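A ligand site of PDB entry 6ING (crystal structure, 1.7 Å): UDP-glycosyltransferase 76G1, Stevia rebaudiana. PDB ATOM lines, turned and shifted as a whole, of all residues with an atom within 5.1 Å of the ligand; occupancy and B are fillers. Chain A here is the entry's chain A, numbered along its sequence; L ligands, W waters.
N of Ser 283 is in hydrogen-bond range of O12 of the ligand (3.0 Å).
The side-chain hydroxyl (OG) of Ser 283 lies within hydrogen-bond range of an oxygen (O12) of the ligand (2.5 Å).
The backbone NH of Ser 361 sits at hydrogen-bond distance from an oxygen (O8) of the ligand (2.9 Å).
OG of Ser 361 lies within hydrogen-bond range of O8 of the ligand (2.5 Å).
The side-chain carboxylate (OE1) of Glu 364 sits at hydrogen-bond distance from an oxygen (O3) of the ligand, at 2.6 Å.
An oxygen (O2) of the ligand is in hydrogen-bond range of the backbone NH of Val 339.
A nitrogen (N2) of the ligand lies within hydrogen-bond range of the backbone carbonyl oxygen (O) of Val 339 (2.6 Å).
O10 of the ligand is in hydrogen-bond range of NE2 of His 356 (2.8 Å).
An oxygen (O7) of the ligand lies within hydrogen-bond range of the backbone NH of Asn 360 (3.2 Å).
The side-chain amide nitrogen (ND2) of Asn 360 sits at hydrogen-bond distance from an oxygen (O7) of the ligand (2.9 Å).
ND2 of Asn 27 sits at hydrogen-bond distance from O5 of the ligand, 3.0 Å away.
N of Gln 341 is in hydrogen-bond range of O1 of the ligand (3.4 Å).
An oxygen (O3) of the ligand lies close to the side-chain amide nitrogen of Gln 341 (3.2 Å).
The side-chain amide nitrogen of Gln 341 is in hydrogen-bond range of the side-chain hydroxyl of Ser 361 (2.9 Å).
OE1 of Glu 364 sits at hydrogen-bond distance from NE2 of Gln 341 (2.8 Å).
The backbone NH of His 356 is in hydrogen-bond range of the backbone carbonyl oxygen of Ser 280 (3.5 Å).
The side-chain amide oxygen of Gln 381 sits close to the backbone carbonyl oxygen of His 356, 3.4 Å away.
The backbone carbonyl oxygen (O) of Gly 24 sits at hydrogen-bond distance from the side-chain amide nitrogen (ND2) of Asn 360.
OD1 of Asn 27 sits at hydrogen-bond distance from NE2 of Gln 23, 2.8 Å away.
The side-chain amide oxygen of Gln 341 is in hydrogen-bond range of the side-chain hydroxyl of Tyr 278 (2.8 Å).
The backbone carbonyl oxygen (O) of Gly 358 is in hydrogen-bond range of the side-chain hydroxyl (OG1) of Thr 362.
Merely in contact with the ligand: Trp 338 (3.3 Å), Val 309 (3.4 Å), Trp 359 (3.6 Å), Gly 358 (3.7 Å), Gln 23 (3.8 Å), Gly 24 (3.8 Å), Tyr 278 (3.9 Å) and Gly 282 (3.95 Å).
Hydrophobic or aromatic side chains within 4 Å of the ligand: Val 309, Trp 338, Val 339 and His 356.
Within 4 Å of the ligand: Gln 23, Gly 24, Asn 27, Tyr 278, Gly 282, Ser 283, Val 309, Trp 338, Val 339, Gln 341, His 356, Gly 358, Trp 359, Asn 360, Ser 361 and Glu 364.
The nearest printed residue that does not touch the ligand is Ser 280 (4.2 Å).
Water W3 lies within hydrogen-bond range of an oxygen (O10) of the ligand (2.6 Å), the side-chain hydroxyl (OG1) of Thr 284 (2.8 Å) and the backbone NH (N) of Ser 283 (3.2 Å).
Water W2 bridges O3 of the ligand and N of Gln 342.
Water W5 bridges N of Gly 24 (2.8 Å) and O11 of the ligand (2.8 Å).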
ATOM      1  N   GLN A  23       4.878   5.964  18.055  1.00  0.00           N
ATOM      2  CA  GLN A  23       3.853   6.717  18.790  1.00  0.00           C
ATOM      3  C   GLN A  23       3.855   8.190  18.413  1.00  0.00           C
ATOM      4  O   GLN A  23       2.784   8.781  18.185  1.00  0.00           O
ATOM      5  CB  GLN A  23       4.069   6.588  20.298  1.00  0.00           C
ATOM      6  CG  GLN A  23       2.865   7.074  21.131  1.00  0.00           C
ATOM      7  CD  GLN A  23       1.722   6.111  21.034  1.00  0.00           C
ATOM      8  OE1 GLN A  23       1.666   5.101  21.751  1.00  0.00           O
ATOM      9  NE2 GLN A  23       0.775   6.407  20.154  1.00  0.00           N
ATOM     10  N   GLY A  24       5.032   8.817  18.390  1.00  0.00           N
ATOM     11  CA  GLY A  24       5.115  10.255  18.098  1.00  0.00           C
ATOM     12  C   GLY A  24       4.809  10.606  16.660  1.00  0.00           C
ATOM     13  O   GLY A  24       4.641  11.788  16.346  1.00  0.00           O
ATOM     14  N   ASN A  27       0.534   9.530  16.356  1.00  0.00           N
ATOM     15  CA  ASN A  27      -0.334  10.455  17.053  1.00  0.00           C
ATOM     16  C   ASN A  27      -0.774  11.631  16.194  1.00  0.00           C
ATOM     17  O   ASN A  27      -1.980  11.838  16.042  1.00  0.00           O
ATOM     18  CB  ASN A  27       0.303  10.925  18.371  1.00  0.00           C
ATOM     19  CG  ASN A  27       0.172   9.858  19.465  1.00  0.00           C
ATOM     20  OD1 ASN A  27      -0.407   8.804  19.233  1.00  0.00           O
ATOM     21  ND2 ASN A  27       0.708  10.130  20.648  1.00  0.00           N
ATOM     22  N   ALA A 252      -4.340  12.755  21.622  1.00  0.00           N
ATOM     23  CA  ALA A 252      -3.984  11.539  20.904  1.00  0.00           C
ATOM     24  C   ALA A 252      -4.301  10.264  21.688  1.00  0.00           C
ATOM     25  O   ALA A 252      -3.698   9.215  21.433  1.00  0.00           O
ATOM     26  CB  ALA A 252      -2.500  11.562  20.531  1.00  0.00           C
ATOM     27  N   TYR A 278       5.130  17.093  36.318  1.00  0.00           N
ATOM     28  CA  TYR A 278       5.044  15.945  35.430  1.00  0.00           C
ATOM     29  C   TYR A 278       6.394  15.770  34.751  1.00  0.00           C
ATOM     30  O   TYR A 278       6.987  16.761  34.311  1.00  0.00           O
ATOM     31  CB  TYR A 278       3.950  16.151  34.385  1.00  0.00           C
ATOM     32  CG  TYR A 278       3.843  15.035  33.357  1.00  0.00           C
ATOM     33  CD1 TYR A 278       3.567  13.735  33.742  1.00  0.00           C
ATOM     34  CD2 TYR A 278       4.086  15.286  32.012  1.00  0.00           C
ATOM     35  CE1 TYR A 278       3.516  12.706  32.808  1.00  0.00           C
ATOM     36  CE2 TYR A 278       4.035  14.266  31.073  1.00  0.00           C
ATOM     37  CZ  TYR A 278       3.740  12.978  31.487  1.00  0.00           C
ATOM     38  OH  TYR A 278       3.680  11.966  30.568  1.00  0.00           O
ATOM     39  N   SER A 280       8.689  13.307  31.997  1.00  0.00           N
ATOM     40  CA  SER A 280       8.755  12.210  31.030  1.00  0.00           C
ATOM     41  C   SER A 280       9.878  12.516  30.049  1.00  0.00           C
ATOM     42  O   SER A 280       9.890  13.593  29.448  1.00  0.00           O
ATOM     43  CB  SER A 280       7.422  12.058  30.291  1.00  0.00           C
ATOM     44  OG  SER A 280       7.540  11.057  29.275  1.00  0.00           O
ATOM     45  N   GLY A 282      10.883  10.542  27.369  1.00  0.00           N
ATOM     46  CA  GLY A 282      10.660  10.192  25.980  1.00  0.00           C
ATOM     47  C   GLY A 282      10.754   8.689  25.723  1.00  0.00           C
ATOM     48  O   GLY A 282      11.189   7.902  26.562  1.00  0.00           O
ATOM     49  N   SER A 283      10.373   8.339  24.489  1.00  0.00           N
ATOM     50  CA  SER A 283      10.158   6.930  24.143  1.00  0.00           C
ATOM     51  C   SER A 283      11.476   6.171  24.009  1.00  0.00           C
ATOM     52  O   SER A 283      11.577   5.009  24.425  1.00  0.00           O
ATOM     53  CB  SER A 283       9.357   6.825  22.842  1.00  0.00           C
ATOM     54  OG  SER A 283       8.125   7.518  22.923  1.00  0.00           O
ATOM     55  N   THR A 284      12.481   6.803  23.422  1.00  0.00           N
ATOM     56  CA  THR A 284      13.717   6.124  23.068  1.00  0.00           C
ATOM     57  C   THR A 284      14.916   6.656  23.840  1.00  0.00           C
ATOM     58  O   THR A 284      16.022   6.106  23.698  1.00  0.00           O
ATOM     59  CB  THR A 284      13.972   6.251  21.566  1.00  0.00           C
ATOM     60  OG1 THR A 284      14.241   7.619  21.219  1.00  0.00           O
ATOM     61  CG2 THR A 284      12.745   5.789  20.780  1.00  0.00           C
ATOM     62  N   VAL A 309       6.860   9.471  34.385  1.00  0.00           N
ATOM     63  CA  VAL A 309       6.735   8.354  33.465  1.00  0.00           C
ATOM     64  C   VAL A 309       8.139   7.892  33.076  1.00  0.00           C
ATOM     65  O   VAL A 309       8.898   8.646  32.452  1.00  0.00           O
ATOM     66  CB  VAL A 309       5.934   8.748  32.210  1.00  0.00           C
ATOM     67  CG1 VAL A 309       5.926   7.595  31.203  1.00  0.00           C
ATOM     68  CG2 VAL A 309       4.516   9.137  32.574  1.00  0.00           C
ATOM     69  N   LYS A 337       4.483   3.846  34.166  1.00  0.00           N
ATOM     70  CA  LYS A 337       5.031   3.462  32.868  1.00  0.00           C
ATOM     71  C   LYS A 337       4.394   4.163  31.673  1.00  0.00           C
ATOM     72  O   LYS A 337       5.049   4.293  30.637  1.00  0.00           O
ATOM     73  CB  LYS A 337       4.904   1.950  32.654  1.00  0.00           C
ATOM     74  CG  LYS A 337       5.662   1.117  33.681  1.00  0.00           C
ATOM     75  CD  LYS A 337       5.765  -0.335  33.276  1.00  0.00           C
ATOM     76  CE  LYS A 337       6.454  -1.144  34.361  1.00  0.00           C
ATOM     77  NZ  LYS A 337       6.459  -2.595  34.066  1.00  0.00           N
ATOM     78  N   TRP A 338       3.132   4.589  31.781  1.00  0.00           N
ATOM     79  CA  TRP A 338       2.412   5.166  30.647  1.00  0.00           C
ATOM     80  C   TRP A 338       1.159   5.845  31.141  1.00  0.00           C
ATOM     81  O   TRP A 338       0.443   5.297  31.974  1.00  0.00           O
ATOM     82  CB  TRP A 338       2.057   4.097  29.610  1.00  0.00           C
ATOM     83  CG  TRP A 338       1.592   4.638  28.319  1.00  0.00           C
ATOM     84  CD1 TRP A 338       0.320   4.631  27.822  1.00  0.00           C
ATOM     85  CD2 TRP A 338       2.389   5.293  27.324  1.00  0.00           C
ATOM     86  NE1 TRP A 338       0.278   5.220  26.583  1.00  0.00           N
ATOM     87  CE2 TRP A 338       1.540   5.644  26.259  1.00  0.00           C
ATOM     88  CE3 TRP A 338       3.742   5.625  27.246  1.00  0.00           C
ATOM     89  CZ2 TRP A 338       2.004   6.287  25.121  1.00  0.00           C
ATOM     90  CZ3 TRP A 338       4.205   6.262  26.089  1.00  0.00           C
ATOM     91  CH2 TRP A 338       3.336   6.583  25.057  1.00  0.00           C
ATOM     92  N   VAL A 339       0.917   7.053  30.638  1.00  0.00           N
ATOM     93  CA  VAL A 339      -0.286   7.803  30.985  1.00  0.00           C
ATOM     94  C   VAL A 339      -0.898   8.392  29.724  1.00  0.00           C
ATOM     95  O   VAL A 339      -0.261   8.363  28.663  1.00  0.00           O
ATOM     96  CB  VAL A 339       0.021   8.916  31.996  1.00  0.00           C
ATOM     97  CG1 VAL A 339       0.764   8.380  33.211  1.00  0.00           C
ATOM     98  CG2 VAL A 339       0.824  10.062  31.308  1.00  0.00           C
ATOM     99  N   PRO A 340      -2.127   8.907  29.787  1.00  0.00           N
ATOM    100  CA  PRO A 340      -2.636   9.740  28.698  1.00  0.00           C
ATOM    101  C   PRO A 340      -2.045  11.133  28.865  1.00  0.00           C
ATOM    102  O   PRO A 340      -2.547  11.934  29.660  1.00  0.00           O
ATOM    103  CB  PRO A 340      -4.155   9.729  28.874  1.00  0.00           C
ATOM    104  CG  PRO A 340      -4.414   9.083  30.220  1.00  0.00           C
ATOM    105  CD  PRO A 340      -3.098   8.831  30.910  1.00  0.00           C
ATOM    106  N   GLN A 341      -0.956  11.430  28.167  1.00  0.00           N
ATOM    107  CA  GLN A 341      -0.092  12.519  28.600  1.00  0.00           C
ATOM    108  C   GLN A 341      -0.799  13.868  28.510  1.00  0.00           C
ATOM    109  O   GLN A 341      -0.687  14.694  29.423  1.00  0.00           O
ATOM    110  CB  GLN A 341       1.174  12.554  27.760  1.00  0.00           C
ATOM    111  CG  GLN A 341       1.971  13.827  27.997  1.00  0.00           C
ATOM    112  CD  GLN A 341       3.387  13.709  27.445  1.00  0.00           C
ATOM    113  OE1 GLN A 341       4.217  12.941  27.974  1.00  0.00           O
ATOM    114  NE2 GLN A 341       3.675  14.439  26.376  1.00  0.00           N
ATOM    115  N   GLN A 342      -1.472  14.143  27.402  1.00  0.00           N
ATOM    116  CA  GLN A 342      -2.060  15.476  27.281  1.00  0.00           C
ATOM    117  C   GLN A 342      -3.172  15.663  28.321  1.00  0.00           C
ATOM    118  O   GLN A 342      -3.337  16.747  28.878  1.00  0.00           O
ATOM    119  CB  GLN A 342      -2.590  15.717  25.871  1.00  0.00           C
ATOM    120  CG  GLN A 342      -3.025  17.171  25.688  1.00  0.00           C
ATOM    121  CD  GLN A 342      -3.438  17.539  24.312  1.00  0.00           C
ATOM    122  OE1 GLN A 342      -3.156  16.842  23.378  1.00  0.00           O
ATOM    123  NE2 GLN A 342      -4.096  18.665  24.176  1.00  0.00           N
ATOM    124  N   HIS A 356      11.769  15.912  27.633  1.00  0.00           N
ATOM    125  CA  HIS A 356      12.915  15.733  26.728  1.00  0.00           C
ATOM    126  C   HIS A 356      12.836  16.626  25.494  1.00  0.00           C
ATOM    127  O   HIS A 356      13.749  16.611  24.663  1.00  0.00           O
ATOM    128  CB  HIS A 356      13.036  14.267  26.317  1.00  0.00           C
ATOM    129  CG  HIS A 356      12.026  13.809  25.307  1.00  0.00           C
ATOM    130  ND1 HIS A 356      10.665  13.996  25.457  1.00  0.00           N
ATOM    131  CD2 HIS A 356      12.194  13.141  24.131  1.00  0.00           C
ATOM    132  CE1 HIS A 356      10.041  13.462  24.419  1.00  0.00           C
ATOM    133  NE2 HIS A 356      10.943  12.919  23.608  1.00  0.00           N
ATOM    134  N   GLY A 358      10.735  16.497  22.921  1.00  0.00           N
ATOM    135  CA  GLY A 358      10.110  16.022  21.701  1.00  0.00           C
ATOM    136  C   GLY A 358       8.999  16.952  21.292  1.00  0.00           C
ATOM    137  O   GLY A 358       8.383  17.642  22.123  1.00  0.00           O
ATOM    138  N   TRP A 359       8.745  17.037  19.974  1.00  0.00           N
ATOM    139  CA  TRP A 359       7.836  18.060  19.490  1.00  0.00           C
ATOM    140  C   TRP A 359       6.394  17.835  19.927  1.00  0.00           C
ATOM    141  O   TRP A 359       5.711  18.803  20.302  1.00  0.00           O
ATOM    142  CB  TRP A 359       7.879  18.175  17.968  1.00  0.00           C
ATOM    143  CG  TRP A 359       7.097  19.355  17.484  1.00  0.00           C
ATOM    144  CD1 TRP A 359       6.008  19.336  16.664  1.00  0.00           C
ATOM    145  CD2 TRP A 359       7.301  20.742  17.828  1.00  0.00           C
ATOM    146  NE1 TRP A 359       5.554  20.590  16.461  1.00  0.00           N
ATOM    147  CE2 TRP A 359       6.316  21.486  17.164  1.00  0.00           C
ATOM    148  CE3 TRP A 359       8.255  21.420  18.596  1.00  0.00           C
ATOM    149  CZ2 TRP A 359       6.264  22.872  17.229  1.00  0.00           C
ATOM    150  CZ3 TRP A 359       8.143  22.786  18.713  1.00  0.00           C
ATOM    151  CH2 TRP A 359       7.167  23.496  18.019  1.00  0.00           C
ATOM    152  N   ASN A 360       5.871  16.598  19.838  1.00  0.00           N
ATOM    153  CA  ASN A 360       4.501  16.395  20.339  1.00  0.00           C
ATOM    154  C   ASN A 360       4.379  16.835  21.792  1.00  0.00           C
ATOM    155  O   ASN A 360       3.414  17.513  22.169  1.00  0.00           O
ATOM    156  CB  ASN A 360       4.039  14.945  20.200  1.00  0.00           C
ATOM    157  CG  ASN A 360       3.931  14.514  18.751  1.00  0.00           C
ATOM    158  OD1 ASN A 360       3.034  14.969  18.011  1.00  0.00           O
ATOM    159  ND2 ASN A 360       4.858  13.658  18.325  1.00  0.00           N
ATOM    160  N   SER A 361       5.311  16.412  22.647  1.00  0.00           N
ATOM    161  CA  SER A 361       5.213  16.741  24.066  1.00  0.00           C
ATOM    162  C   SER A 361       5.290  18.249  24.294  1.00  0.00           C
ATOM    163  O   SER A 361       4.548  18.798  25.108  1.00  0.00           O
ATOM    164  CB  SER A 361       6.333  16.065  24.861  1.00  0.00           C
ATOM    165  OG  SER A 361       6.167  14.677  24.912  1.00  0.00           O
ATOM    166  N   THR A 362       6.224  18.915  23.622  1.00  0.00           N
ATOM    167  CA  THR A 362       6.376  20.372  23.749  1.00  0.00           C
ATOM    168  C   THR A 362       5.106  21.089  23.330  1.00  0.00           C
ATOM    169  O   THR A 362       4.585  21.957  24.047  1.00  0.00           O
ATOM    170  CB  THR A 362       7.549  20.834  22.900  1.00  0.00           C
ATOM    171  OG1 THR A 362       8.742  20.171  23.344  1.00  0.00           O
ATOM    172  CG2 THR A 362       7.723  22.330  23.021  1.00  0.00           C
ATOM    173  N   GLU A 364       2.044  19.798  23.074  1.00  0.00           N
ATOM    174  CA  GLU A 364       0.970  19.488  24.023  1.00  0.00           C
ATOM    175  C   GLU A 364       1.052  20.388  25.241  1.00  0.00           C
ATOM    176  O   GLU A 364       0.054  20.951  25.705  1.00  0.00           O
ATOM    177  CB  GLU A 364       1.048  18.004  24.433  1.00  0.00           C
ATOM    178  CG  GLU A 364       0.616  17.059  23.320  1.00  0.00           C
ATOM    179  CD  GLU A 364       1.202  15.657  23.456  1.00  0.00           C
ATOM    180  OE1 GLU A 364       1.709  15.265  24.550  1.00  0.00           O
ATOM    181  OE2 GLU A 364       1.152  14.921  22.474  1.00  0.00           O
ATOM    182  N   GLN A 381      15.445  17.848  19.510  1.00  0.00           N
ATOM    183  CA  GLN A 381      15.128  18.213  20.892  1.00  0.00           C
ATOM    184  C   GLN A 381      15.909  19.410  21.404  1.00  0.00           C
ATOM    185  O   GLN A 381      15.307  20.275  22.050  1.00  0.00           O
ATOM    186  CB  GLN A 381      15.347  16.993  21.785  1.00  0.00           C
ATOM    187  CG  GLN A 381      14.355  15.906  21.485  1.00  0.00           C
ATOM    188  CD  GLN A 381      14.770  14.540  21.956  1.00  0.00           C
ATOM    189  OE1 GLN A 381      15.543  14.372  22.901  1.00  0.00           O
ATOM    190  NE2 GLN A 381      14.205  13.539  21.329  1.00  0.00           N
HETATM  191  N1  LIG L   1       2.844   9.986  25.517  1.00  0.00           N
HETATM  192  C1  LIG L   1       1.727   9.513  26.175  1.00  0.00           C
HETATM  193  N2  LIG L   1       1.952   8.986  27.426  1.00  0.00           N
HETATM  194  C2  LIG L   1       3.180   8.849  28.044  1.00  0.00           C
HETATM  195  C3  LIG L   1       4.288   9.379  27.311  1.00  0.00           C
HETATM  196  C4  LIG L   1       4.084   9.902  26.081  1.00  0.00           C
HETATM  197  O1  LIG L   1       0.600   9.608  25.709  1.00  0.00           O
HETATM  198  O2  LIG L   1       3.233   8.340  29.188  1.00  0.00           O
HETATM  199  C5  LIG L   1       2.661  10.571  24.199  1.00  0.00           C
HETATM  200  C6  LIG L   1       2.853  12.084  24.196  1.00  0.00           C
HETATM  201  O3  LIG L   1       1.625  12.710  24.581  1.00  0.00           O
HETATM  202  C7  LIG L   1       3.223  12.331  22.740  1.00  0.00           C
HETATM  203  C8  LIG L   1       4.056  11.089  22.390  1.00  0.00           C
HETATM  204  O4  LIG L   1       3.663  10.057  23.330  1.00  0.00           O
HETATM  205  O5  LIG L   1       2.090  12.446  21.903  1.00  0.00           O
HETATM  206  C9  LIG L   1       5.540  11.313  22.518  1.00  0.00           C
HETATM  207  O6  LIG L   1       5.957  12.072  21.370  1.00  0.00           O
HETATM  208  P1  LIG L   1       7.162  13.113  21.424  1.00  0.00           P
HETATM  209  O7  LIG L   1       7.201  13.752  20.099  1.00  0.00           O
HETATM  210  O8  LIG L   1       7.025  14.067  22.597  1.00  0.00           O
HETATM  211  O9  LIG L   1       8.486  12.286  21.701  1.00  0.00           O
HETATM  212  P2  LIG L   1       9.072  10.830  21.472  1.00  0.00           P
HETATM  213  O10 LIG L   1      10.574  11.084  21.482  1.00  0.00           O
HETATM  214  O11 LIG L   1       8.528  10.474  20.096  1.00  0.00           O
HETATM  215  O12 LIG L   1       8.657   9.908  22.586  1.00  0.00           O
HETATM  216  O   HOH W   1       7.246  10.353  25.122  1.00  0.00           O
HETATM  217  O   HOH W   2      -1.081  12.779  24.781  1.00  0.00           O
HETATM  218  O   HOH W   3      12.408   9.496  22.307  1.00  0.00           O
HETATM  219  O   HOH W   4      -1.777   8.500  25.263  1.00  0.00           O
HETATM  220  O   HOH W   5       7.451   7.938  19.471  1.00  0.00           O
